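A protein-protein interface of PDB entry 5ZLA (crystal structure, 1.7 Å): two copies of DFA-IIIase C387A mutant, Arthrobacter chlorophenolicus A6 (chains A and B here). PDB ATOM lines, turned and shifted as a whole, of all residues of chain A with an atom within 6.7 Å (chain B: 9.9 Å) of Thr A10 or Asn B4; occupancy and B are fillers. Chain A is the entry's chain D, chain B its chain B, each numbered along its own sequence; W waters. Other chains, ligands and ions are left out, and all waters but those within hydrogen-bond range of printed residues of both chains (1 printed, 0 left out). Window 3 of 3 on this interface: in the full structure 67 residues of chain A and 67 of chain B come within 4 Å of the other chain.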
ATOM      1  N   TYR A   7     -12.833  -9.564 -23.627  1.00  0.00           N
ATOM      2  CA  TYR A   7     -11.834  -8.546 -23.910  1.00  0.00           C
ATOM      3  C   TYR A   7     -12.491  -7.180 -23.997  1.00  0.00           C
ATOM      4  O   TYR A   7     -13.656  -7.056 -24.367  1.00  0.00           O
ATOM      5  CB  TYR A   7     -11.135  -8.822 -25.239  1.00  0.00           C
ATOM      6  CG  TYR A   7     -10.420 -10.150 -25.338  1.00  0.00           C
ATOM      7  CD1 TYR A   7     -11.111 -11.314 -25.652  1.00  0.00           C
ATOM      8  CD2 TYR A   7      -9.037 -10.233 -25.172  1.00  0.00           C
ATOM      9  CE1 TYR A   7     -10.447 -12.529 -25.787  1.00  0.00           C
ATOM     10  CE2 TYR A   7      -8.371 -11.440 -25.280  1.00  0.00           C
ATOM     11  CZ  TYR A   7      -9.073 -12.587 -25.589  1.00  0.00           C
ATOM     12  OH  TYR A   7      -8.389 -13.772 -25.705  1.00  0.00           O
ATOM     13  N   ASP A   8     -11.706  -6.156 -23.696  1.00  0.00           N
ATOM     14  CA  ASP A   8     -12.128  -4.756 -23.813  1.00  0.00           C
ATOM     15  C   ASP A   8     -11.032  -4.072 -24.627  1.00  0.00           C
ATOM     16  O   ASP A   8      -9.858  -4.141 -24.254  1.00  0.00           O
ATOM     17  CB  ASP A   8     -12.266  -4.169 -22.410  1.00  0.00           C
ATOM     18  CG  ASP A   8     -12.665  -2.697 -22.398  1.00  0.00           C
ATOM     19  OD1 ASP A   8     -12.193  -1.906 -23.238  1.00  0.00           O
ATOM     20  OD2 ASP A   8     -13.444  -2.325 -21.500  1.00  0.00           O
ATOM     21  N   VAL A   9     -11.397  -3.420 -25.730  1.00  0.00           N
ATOM     22  CA  VAL A   9     -10.384  -2.851 -26.650  1.00  0.00           C
ATOM     23  C   VAL A   9      -9.531  -1.756 -26.008  1.00  0.00           C
ATOM     24  O   VAL A   9      -8.440  -1.482 -26.503  1.00  0.00           O
ATOM     25  CB  VAL A   9     -10.963  -2.332 -28.002  1.00  0.00           C
ATOM     26  CG1 VAL A   9     -11.635  -3.469 -28.771  1.00  0.00           C
ATOM     27  CG2 VAL A   9     -11.921  -1.158 -27.817  1.00  0.00           C
ATOM     28  N   THR A  10     -10.027  -1.155 -24.921  1.00  0.00           N
ATOM     29  CA  THR A  10      -9.289  -0.143 -24.150  1.00  0.00           C
ATOM     30  C   THR A  10      -8.397  -0.739 -23.052  1.00  0.00           C
ATOM     31  O   THR A  10      -7.673   0.000 -22.399  1.00  0.00           O
ATOM     32  CB  THR A  10     -10.229   0.919 -23.520  1.00  0.00           C
ATOM     33  OG1 THR A  10     -11.024   0.343 -22.471  1.00  0.00           O
ATOM     34  CG2 THR A  10     -11.144   1.540 -24.582  1.00  0.00           C
ATOM     35  N   GLU A  11      -8.443  -2.063 -22.874  1.00  0.00           N
ATOM     36  CA  GLU A  11      -7.647  -2.781 -21.884  1.00  0.00           C
ATOM     37  C   GLU A  11      -6.881  -3.931 -22.549  1.00  0.00           C
ATOM     38  O   GLU A  11      -6.843  -5.057 -22.032  1.00  0.00           O
ATOM     39  CB  GLU A  11      -8.561  -3.365 -20.802  1.00  0.00           C
ATOM     40  CG  GLU A  11      -9.421  -2.357 -20.057  1.00  0.00           C
ATOM     41  CD  GLU A  11     -10.356  -3.016 -19.047  1.00  0.00           C
ATOM     42  OE1 GLU A  11     -10.399  -4.266 -18.981  1.00  0.00           O
ATOM     43  OE2 GLU A  11     -11.057  -2.284 -18.311  1.00  0.00           O
ATOM     44  N   TRP A  12      -6.286  -3.661 -23.703  1.00  0.00           N
ATOM     45  CA  TRP A  12      -5.468  -4.656 -24.398  1.00  0.00           C
ATOM     46  C   TRP A  12      -4.089  -4.036 -24.629  1.00  0.00           C
ATOM     47  O   TRP A  12      -4.000  -3.015 -25.292  1.00  0.00           O
ATOM     48  CB  TRP A  12      -6.125  -5.083 -25.713  1.00  0.00           C
ATOM     49  CG  TRP A  12      -5.409  -6.216 -26.336  1.00  0.00           C
ATOM     50  CD1 TRP A  12      -4.683  -6.189 -27.479  1.00  0.00           C
ATOM     51  CD2 TRP A  12      -5.308  -7.548 -25.819  1.00  0.00           C
ATOM     52  NE1 TRP A  12      -4.143  -7.426 -27.722  1.00  0.00           N
ATOM     53  CE2 TRP A  12      -4.509  -8.281 -26.721  1.00  0.00           C
ATOM     54  CE3 TRP A  12      -5.817  -8.192 -24.688  1.00  0.00           C
ATOM     55  CZ2 TRP A  12      -4.203  -9.636 -26.530  1.00  0.00           C
ATOM     56  CZ3 TRP A  12      -5.507  -9.541 -24.485  1.00  0.00           C
ATOM     57  CH2 TRP A  12      -4.708 -10.248 -25.409  1.00  0.00           C
ATOM     58  N   PRO A  17      -6.467   1.652 -29.484  1.00  0.00           N
ATOM     59  CA  PRO A  17      -7.702   1.645 -30.270  1.00  0.00           C
ATOM     60  C   PRO A  17      -8.134   3.014 -30.809  1.00  0.00           C
ATOM     61  O   PRO A  17      -8.859   3.063 -31.791  1.00  0.00           O
ATOM     62  CB  PRO A  17      -8.733   1.072 -29.289  1.00  0.00           C
ATOM     63  CG  PRO A  17      -8.230   1.464 -27.956  1.00  0.00           C
ATOM     64  CD  PRO A  17      -6.731   1.420 -28.053  1.00  0.00           C
ATOM     65  N   VAL A  24      -5.751  -3.645 -32.854  1.00  0.00           N
ATOM     66  CA  VAL A  24      -6.122  -4.126 -31.518  1.00  0.00           C
ATOM     67  C   VAL A  24      -6.993  -5.382 -31.630  1.00  0.00           C
ATOM     68  O   VAL A  24      -6.710  -6.396 -30.982  1.00  0.00           O
ATOM     69  CB  VAL A  24      -6.837  -3.042 -30.674  1.00  0.00           C
ATOM     70  CG1 VAL A  24      -7.373  -3.618 -29.365  1.00  0.00           C
ATOM     71  CG2 VAL A  24      -5.893  -1.883 -30.379  1.00  0.00           C
ATOM     72  N   TYR A  52     -15.471  -6.178 -26.312  1.00  0.00           N
ATOM     73  CA  TYR A  52     -16.287  -5.013 -25.945  1.00  0.00           C
ATOM     74  C   TYR A  52     -15.605  -3.696 -26.340  1.00  0.00           C
ATOM     75  O   TYR A  52     -14.408  -3.493 -26.099  1.00  0.00           O
ATOM     76  CB  TYR A  52     -16.584  -5.029 -24.437  1.00  0.00           C
ATOM     77  CG  TYR A  52     -17.323  -3.804 -23.947  1.00  0.00           C
ATOM     78  CD1 TYR A  52     -18.582  -3.498 -24.452  1.00  0.00           C
ATOM     79  CD2 TYR A  52     -16.789  -2.963 -22.970  1.00  0.00           C
ATOM     80  CE1 TYR A  52     -19.282  -2.392 -24.023  1.00  0.00           C
ATOM     81  CE2 TYR A  52     -17.494  -1.850 -22.523  1.00  0.00           C
ATOM     82  CZ  TYR A  52     -18.733  -1.565 -23.071  1.00  0.00           C
ATOM     83  OH  TYR A  52     -19.456  -0.474 -22.660  1.00  0.00           O
ATOM     84  N   LEU A  53     -16.393  -2.820 -26.942  1.00  0.00           N
ATOM     85  CA  LEU A  53     -16.002  -1.461 -27.321  1.00  0.00           C
ATOM     86  C   LEU A  53     -16.799  -0.502 -26.451  1.00  0.00           C
ATOM     87  O   LEU A  53     -17.987  -0.302 -26.695  1.00  0.00           O
ATOM     88  CB  LEU A  53     -16.354  -1.181 -28.775  1.00  0.00           C
ATOM     89  CG  LEU A  53     -15.444  -1.747 -29.861  1.00  0.00           C
ATOM     90  CD1 LEU A  53     -15.434  -3.271 -29.855  1.00  0.00           C
ATOM     91  CD2 LEU A  53     -15.891  -1.192 -31.196  1.00  0.00           C
ATOM     92  N   PRO A  54     -16.160   0.100 -25.439  1.00  0.00           N
ATOM     93  CA  PRO A  54     -16.820   1.177 -24.691  1.00  0.00           C
ATOM     94  C   PRO A  54     -17.128   2.350 -25.627  1.00  0.00           C
ATOM     95  O   PRO A  54     -16.508   2.454 -26.679  1.00  0.00           O
ATOM     96  CB  PRO A  54     -15.755   1.604 -23.664  1.00  0.00           C
ATOM     97  CG  PRO A  54     -14.750   0.506 -23.625  1.00  0.00           C
ATOM     98  CD  PRO A  54     -14.788  -0.160 -24.960  1.00  0.00           C
ATOM     99  N   PRO A  55     -18.070   3.233 -25.259  1.00  0.00           N
ATOM    100  CA  PRO A  55     -18.278   4.440 -26.074  1.00  0.00           C
ATOM    101  C   PRO A  55     -16.963   5.194 -26.245  1.00  0.00           C
ATOM    102  O   PRO A  55     -16.191   5.305 -25.294  1.00  0.00           O
ATOM    103  CB  PRO A  55     -19.283   5.253 -25.261  1.00  0.00           C
ATOM    104  CG  PRO A  55     -19.993   4.221 -24.436  1.00  0.00           C
ATOM    105  CD  PRO A  55     -18.949   3.213 -24.086  1.00  0.00           C
ATOM    106  N   GLY A  56     -16.698   5.636 -27.463  1.00  0.00           N
ATOM    107  CA  GLY A  56     -15.411   6.249 -27.800  1.00  0.00           C
ATOM    108  C   GLY A  56     -15.249   6.390 -29.297  1.00  0.00           C
ATOM    109  O   GLY A  56     -16.015   5.805 -30.084  1.00  0.00           O
ATOM    110  N   TYR A  58     -12.870   5.546 -32.197  1.00  0.00           N
ATOM    111  CA  TYR A  58     -11.804   4.601 -32.544  1.00  0.00           C
ATOM    112  C   TYR A  58     -11.499   4.624 -34.032  1.00  0.00           C
ATOM    113  O   TYR A  58     -12.330   4.255 -34.834  1.00  0.00           O
ATOM    114  CB  TYR A  58     -12.224   3.169 -32.145  1.00  0.00           C
ATOM    115  CG  TYR A  58     -12.684   3.039 -30.710  1.00  0.00           C
ATOM    116  CD1 TYR A  58     -11.796   3.222 -29.651  1.00  0.00           C
ATOM    117  CD2 TYR A  58     -14.008   2.739 -30.401  1.00  0.00           C
ATOM    118  CE1 TYR A  58     -12.202   3.087 -28.332  1.00  0.00           C
ATOM    119  CE2 TYR A  58     -14.422   2.612 -29.085  1.00  0.00           C
ATOM    120  CZ  TYR A  58     -13.524   2.793 -28.053  1.00  0.00           C
ATOM    121  OH  TYR A  58     -13.913   2.669 -26.738  1.00  0.00           O
ATOM    122  N   SER B   3     -10.594   8.185 -18.913  1.00  0.00           N
ATOM    123  CA  SER B   3     -11.863   7.404 -18.812  1.00  0.00           C
ATOM    124  C   SER B   3     -12.218   6.741 -20.142  1.00  0.00           C
ATOM    125  O   SER B   3     -11.945   7.277 -21.227  1.00  0.00           O
ATOM    126  CB  SER B   3     -13.027   8.283 -18.332  1.00  0.00           C
ATOM    127  OG  SER B   3     -14.300   7.711 -18.621  1.00  0.00           O
ATOM    128  N   ASN B   4     -12.840   5.574 -20.026  1.00  0.00           N
ATOM    129  CA  ASN B   4     -13.391   4.853 -21.182  1.00  0.00           C
ATOM    130  C   ASN B   4     -14.889   5.118 -21.375  1.00  0.00           C
ATOM    131  O   ASN B   4     -15.540   4.377 -22.107  1.00  0.00           O
ATOM    132  CB  ASN B   4     -13.111   3.337 -21.080  1.00  0.00           C
ATOM    133  CG  ASN B   4     -13.437   2.742 -19.714  1.00  0.00           C
ATOM    134  OD1 ASN B   4     -12.777   1.803 -19.287  1.00  0.00           O
ATOM    135  ND2 ASN B   4     -14.442   3.282 -19.019  1.00  0.00           N
ATOM    136  N   ASN B   5     -15.441   6.144 -20.694  1.00  0.00           N
ATOM    137  CA  ASN B   5     -16.860   6.532 -20.871  1.00  0.00           C
ATOM    138  C   ASN B   5     -17.894   5.498 -20.398  1.00  0.00           C
ATOM    139  O   ASN B   5     -19.044   5.510 -20.853  1.00  0.00           O
ATOM    140  CB  ASN B   5     -17.142   6.918 -22.330  1.00  0.00           C
ATOM    141  CG  ASN B   5     -16.230   8.011 -22.819  1.00  0.00           C
ATOM    142  OD1 ASN B   5     -16.101   9.042 -22.161  1.00  0.00           O
ATOM    143  ND2 ASN B   5     -15.607   7.815 -23.964  1.00  0.00           N
ATOM    144  N   ARG B   6     -17.503   4.649 -19.456  1.00  0.00           N
ATOM    145  CA  ARG B   6     -18.389   3.643 -18.880  1.00  0.00           C
ATOM    146  C   ARG B   6     -18.467   3.931 -17.380  1.00  0.00           C
ATOM    147  O   ARG B   6     -17.435   4.023 -16.704  1.00  0.00           O
ATOM    148  CB  ARG B   6     -17.894   2.200 -19.165  1.00  0.00           C
ATOM    149  CG  ARG B   6     -18.841   1.153 -18.592  1.00  0.00           C
ATOM    150  CD  ARG B   6     -18.634  -0.262 -19.114  1.00  0.00           C
ATOM    151  NE  ARG B   6     -19.670  -1.080 -18.481  1.00  0.00           N
ATOM    152  CZ  ARG B   6     -20.915  -1.272 -18.935  1.00  0.00           C
ATOM    153  NH1 ARG B   6     -21.322  -0.785 -20.110  1.00  0.00           N
ATOM    154  NH2 ARG B   6     -21.762  -1.995 -18.209  1.00  0.00           N
ATOM    155  N   TYR B   7     -19.694   4.091 -16.880  1.00  0.00           N
ATOM    156  CA  TYR B   7     -19.952   4.369 -15.477  1.00  0.00           C
ATOM    157  C   TYR B   7     -20.910   3.348 -14.891  1.00  0.00           C
ATOM    158  O   TYR B   7     -21.775   2.819 -15.590  1.00  0.00           O
ATOM    159  CB  TYR B   7     -20.581   5.745 -15.329  1.00  0.00           C
ATOM    160  CG  TYR B   7     -19.763   6.894 -15.867  1.00  0.00           C
ATOM    161  CD1 TYR B   7     -19.786   7.225 -17.222  1.00  0.00           C
ATOM    162  CD2 TYR B   7     -19.005   7.690 -15.008  1.00  0.00           C
ATOM    163  CE1 TYR B   7     -19.069   8.311 -17.720  1.00  0.00           C
ATOM    164  CE2 TYR B   7     -18.278   8.778 -15.494  1.00  0.00           C
ATOM    165  CZ  TYR B   7     -18.310   9.085 -16.849  1.00  0.00           C
ATOM    166  OH  TYR B   7     -17.608  10.163 -17.326  1.00  0.00           O
ATOM    167  N   ASP B   8     -20.760   3.103 -13.595  1.00  0.00           N
ATOM    168  CA  ASP B   8     -21.634   2.225 -12.838  1.00  0.00           C
ATOM    169  C   ASP B   8     -22.116   3.072 -11.660  1.00  0.00           C
ATOM    170  O   ASP B   8     -21.313   3.611 -10.900  1.00  0.00           O
ATOM    171  CB  ASP B   8     -20.860   0.967 -12.436  1.00  0.00           C
ATOM    172  CG  ASP B   8     -21.655  -0.005 -11.577  1.00  0.00           C
ATOM    173  OD1 ASP B   8     -22.483   0.410 -10.760  1.00  0.00           O
ATOM    174  OD2 ASP B   8     -21.411  -1.225 -11.677  1.00  0.00           O
ATOM    175  N   GLU B  11     -20.598   2.572  -8.310  1.00  0.00           N
ATOM    176  CA  GLU B  11     -19.151   2.835  -8.241  1.00  0.00           C
ATOM    177  C   GLU B  11     -18.880   4.304  -8.530  1.00  0.00           C
ATOM    178  O   GLU B  11     -18.034   4.629  -9.351  1.00  0.00           O
ATOM    179  CB  GLU B  11     -18.403   1.952  -9.247  1.00  0.00           C
ATOM    180  CG  GLU B  11     -18.708   0.467  -9.073  1.00  0.00           C
ATOM    181  CD  GLU B  11     -17.924  -0.444 -10.007  1.00  0.00           C
ATOM    182  OE1 GLU B  11     -17.213   0.052 -10.906  1.00  0.00           O
ATOM    183  OE2 GLU B  11     -18.016  -1.679  -9.831  1.00  0.00           O
ATOM    184  N   ASP B  31     -19.632  15.041 -15.403  1.00  0.00           N
ATOM    185  CA  ASP B  31     -18.292  14.515 -15.693  1.00  0.00           C
ATOM    186  C   ASP B  31     -18.091  14.235 -17.181  1.00  0.00           C
ATOM    187  O   ASP B  31     -17.036  14.563 -17.732  1.00  0.00           O
ATOM    188  CB  ASP B  31     -18.018  13.256 -14.876  1.00  0.00           C
ATOM    189  CG  ASP B  31     -16.584  12.784 -15.002  1.00  0.00           C
ATOM    190  OD1 ASP B  31     -15.680  13.466 -14.462  1.00  0.00           O
ATOM    191  OD2 ASP B  31     -16.362  11.731 -15.636  1.00  0.00           O
ATOM    192  N   ILE B  32     -19.098  13.634 -17.829  1.00  0.00           N
ATOM    193  CA  ILE B  32     -19.030  13.385 -19.267  1.00  0.00           C
ATOM    194  C   ILE B  32     -18.807  14.710 -20.014  1.00  0.00           C
ATOM    195  O   ILE B  32     -17.899  14.823 -20.850  1.00  0.00           O
ATOM    196  CB  ILE B  32     -20.290  12.651 -19.805  1.00  0.00           C
ATOM    197  CG1 ILE B  32     -20.394  11.251 -19.178  1.00  0.00           C
ATOM    198  CG2 ILE B  32     -20.233  12.542 -21.328  1.00  0.00           C
ATOM    199  CD1 ILE B  32     -21.778  10.674 -19.211  1.00  0.00           C
ATOM    200  N   ARG B  35     -15.316  16.257 -19.628  1.00  0.00           N
ATOM    201  CA  ARG B  35     -14.303  15.541 -20.401  1.00  0.00           C
ATOM    202  C   ARG B  35     -14.493  15.668 -21.916  1.00  0.00           C
ATOM    203  O   ARG B  35     -13.507  15.642 -22.642  1.00  0.00           O
ATOM    204  CB  ARG B  35     -14.273  14.062 -19.997  1.00  0.00           C
ATOM    205  CG  ARG B  35     -13.980  13.779 -18.512  1.00  0.00           C
ATOM    206  CD  ARG B  35     -14.480  12.388 -18.104  1.00  0.00           C
ATOM    207  NE  ARG B  35     -14.118  11.491 -19.171  1.00  0.00           N
ATOM    208  CZ  ARG B  35     -14.923  10.736 -19.926  1.00  0.00           C
ATOM    209  NH1 ARG B  35     -16.246  10.575 -19.711  1.00  0.00           N
ATOM    210  NH2 ARG B  35     -14.340  10.050 -20.894  1.00  0.00           N
ATOM    211  N   GLN B  36     -15.742  15.804 -22.389  1.00  0.00           N
ATOM    212  CA  GLN B  36     -16.072  15.855 -23.820  1.00  0.00           C
ATOM    213  C   GLN B  36     -16.527  17.254 -24.262  1.00  0.00           C
ATOM    214  O   GLN B  36     -17.679  17.468 -24.656  1.00  0.00           O
ATOM    215  CB  GLN B  36     -17.141  14.806 -24.159  1.00  0.00           C
ATOM    216  CG  GLN B  36     -16.705  13.390 -23.806  1.00  0.00           C
ATOM    217  CD  GLN B  36     -17.692  12.325 -24.256  1.00  0.00           C
ATOM    218  OE1 GLN B  36     -18.654  12.602 -24.973  1.00  0.00           O
ATOM    219  NE2 GLN B  36     -17.438  11.088 -23.855  1.00  0.00           N
ATOM    220  N   PRO B  47     -18.234  11.464 -28.107  1.00  0.00           N
ATOM    221  CA  PRO B  47     -18.853  10.155 -28.381  1.00  0.00           C
ATOM    222  C   PRO B  47     -19.939   9.718 -27.385  1.00  0.00           C
ATOM    223  O   PRO B  47     -20.624   8.727 -27.631  1.00  0.00           O
ATOM    224  CB  PRO B  47     -17.661   9.205 -28.315  1.00  0.00           C
ATOM    225  CG  PRO B  47     -16.751   9.839 -27.318  1.00  0.00           C
ATOM    226  CD  PRO B  47     -16.858  11.312 -27.606  1.00  0.00           C
ATOM    227  N   GLY B  48     -20.100  10.424 -26.277  1.00  0.00           N
ATOM    228  CA  GLY B  48     -21.098  10.067 -25.281  1.00  0.00           C
ATOM    229  C   GLY B  48     -20.556   9.041 -24.315  1.00  0.00           C
ATOM    230  O   GLY B  48     -19.346   8.994 -24.064  1.00  0.00           O
ATOM    231  N   ALA B  49     -21.450   8.219 -23.762  1.00  0.00           N
ATOM    232  CA  ALA B  49     -21.083   7.364 -22.642  1.00  0.00           C
ATOM    233  C   ALA B  49     -22.185   6.380 -22.365  1.00  0.00           C
ATOM    234  O   ALA B  49     -23.292   6.480 -22.946  1.00  0.00           O
ATOM    235  CB  ALA B  49     -20.821   8.194 -21.384  1.00  0.00           C
ATOM    236  N   VAL B  50     -21.869   5.430 -21.498  1.00  0.00           N
ATOM    237  CA  VAL B  50     -22.860   4.498 -20.979  1.00  0.00           C
ATOM    238  C   VAL B  50     -22.875   4.510 -19.452  1.00  0.00           C
ATOM    239  O   VAL B  50     -21.811   4.532 -18.798  1.00  0.00           O
ATOM    240  CB  VAL B  50     -22.661   3.078 -21.545  1.00  0.00           C
ATOM    241  CG1 VAL B  50     -21.292   2.503 -21.235  1.00  0.00           C
ATOM    242  CG2 VAL B  50     -23.770   2.145 -21.075  1.00  0.00           C
ATOM    243  N   ILE B  51     -24.087   4.513 -18.892  1.00  0.00           N
ATOM    244  CA  ILE B  51     -24.303   4.515 -17.457  1.00  0.00           C
ATOM    245  C   ILE B  51     -25.042   3.231 -17.125  1.00  0.00           C
ATOM    246  O   ILE B  51     -26.156   3.004 -17.618  1.00  0.00           O
ATOM    247  CB  ILE B  51     -25.127   5.738 -16.990  1.00  0.00           C
ATOM    248  CG1 ILE B  51     -24.398   7.042 -17.375  1.00  0.00           C
ATOM    249  CG2 ILE B  51     -25.399   5.649 -15.498  1.00  0.00           C
ATOM    250  CD1 ILE B  51     -25.165   8.318 -17.065  1.00  0.00           C
HETATM  251  O   HOH W   1     -13.404   4.511 -24.774  1.00  0.00           O
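The backbone carbonyl oxygen (O) of Pro A55 lies close to the backbone carbonyl oxygen (O) of Asn B4 (3.4 Å). The guanidinium group (NH1) of Arg B6 lies within hydrogen-bond range of the side-chain hydroxyl (OH) of Tyr A52, 3.2 Å away. O of Pro A55 is in hydrogen-bond range of ND2 of Asn B5.
Among the printed residues, pairs that only touch across the chains: Pro A54 with Asn B4 (3.2 Å), Pro A55 with Val B50 (3.7 Å), Pro A55 with Ala B49 (3.7 Å), Gly A56 with Pro B47 (3.8 Å), Tyr A52 with Val B50 (3.8 Å), Thr A10 with Asn B4 (3.9 Å) and Pro A55 with Gly B48 (3.9 Å).
Positions printed for both chains: 7, 8 and 11. Of the 10 pairs that touch across the chains among the printed residues, none has its exchanged pair printed and touching as well.
Water W1 lies within hydrogen-bond range of OH of Tyr A58, O of Pro A55 and O of Asn B4.
The backbone carbonyl oxygen of Asn B5 is in hydrogen-bond range of the backbone NH of Val B50 (2.9 Å). O of Pro A54 sits at hydrogen-bond distance from OH of Tyr A58 (2.6 Å). OG1 of Thr A10 sits at hydrogen-bond distance from OD1 of Asp A8, 2.6 Å away. The backbone NH (N) of Tyr A52 is in hydrogen-bond range of the backbone carbonyl oxygen (O) of Tyr A7 (2.8 Å). The side-chain amide oxygen of Asn B5 lies within hydrogen-bond range of the side-chain amide nitrogen of Gln B36 (3.0 Å). The backbone NH (N) of Val A9 lies within hydrogen-bond range of the backbone carbonyl oxygen (O) of Tyr A52 (3.0 Å).
Of the 14 printed residues of chain A, 5 touch a printed residue of chain B. Hydrophobic or aromatic side chains of chain A that line the printed part of chain B: Tyr A52, Pro A54 and Pro A55. Printed residues of chain B that touch a printed residue of chain A: Asn B4, Asn B5, Arg B6, Pro B47, Gly B48, Ala B49 and Val B50. Among the printed residues, no Asp or Glu carboxylate lies within 4 Å of a Lys or Arg side-chain nitrogen of the other chain.
Of chain A, only Thr A10, Pro A54 and Pro A55 come within 4 Å of Asn B4. No residue of chain B comes within 4 Å of Asp A8. No residue of chain B comes within 4 Å of Val A9. Of the printed residues of chain A, Gly B48 touches Pro A55. Of the printed residues of chain A, Ala B49 touches Pro A55. Printed residues of chain A within 4 Å of Val B50: Tyr A52 (3.8 Å) and Pro A55 (3.7 Å). Printed residues of chain B within 4 Å of Tyr A52: Arg B6 (3.2 Å) and Val B50 (3.8 Å). Tyr B7 touches none of the printed residues of chain A. The nearest residue of chain B that does not touch Thr A10 is Ser B3 (6.7 Å).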
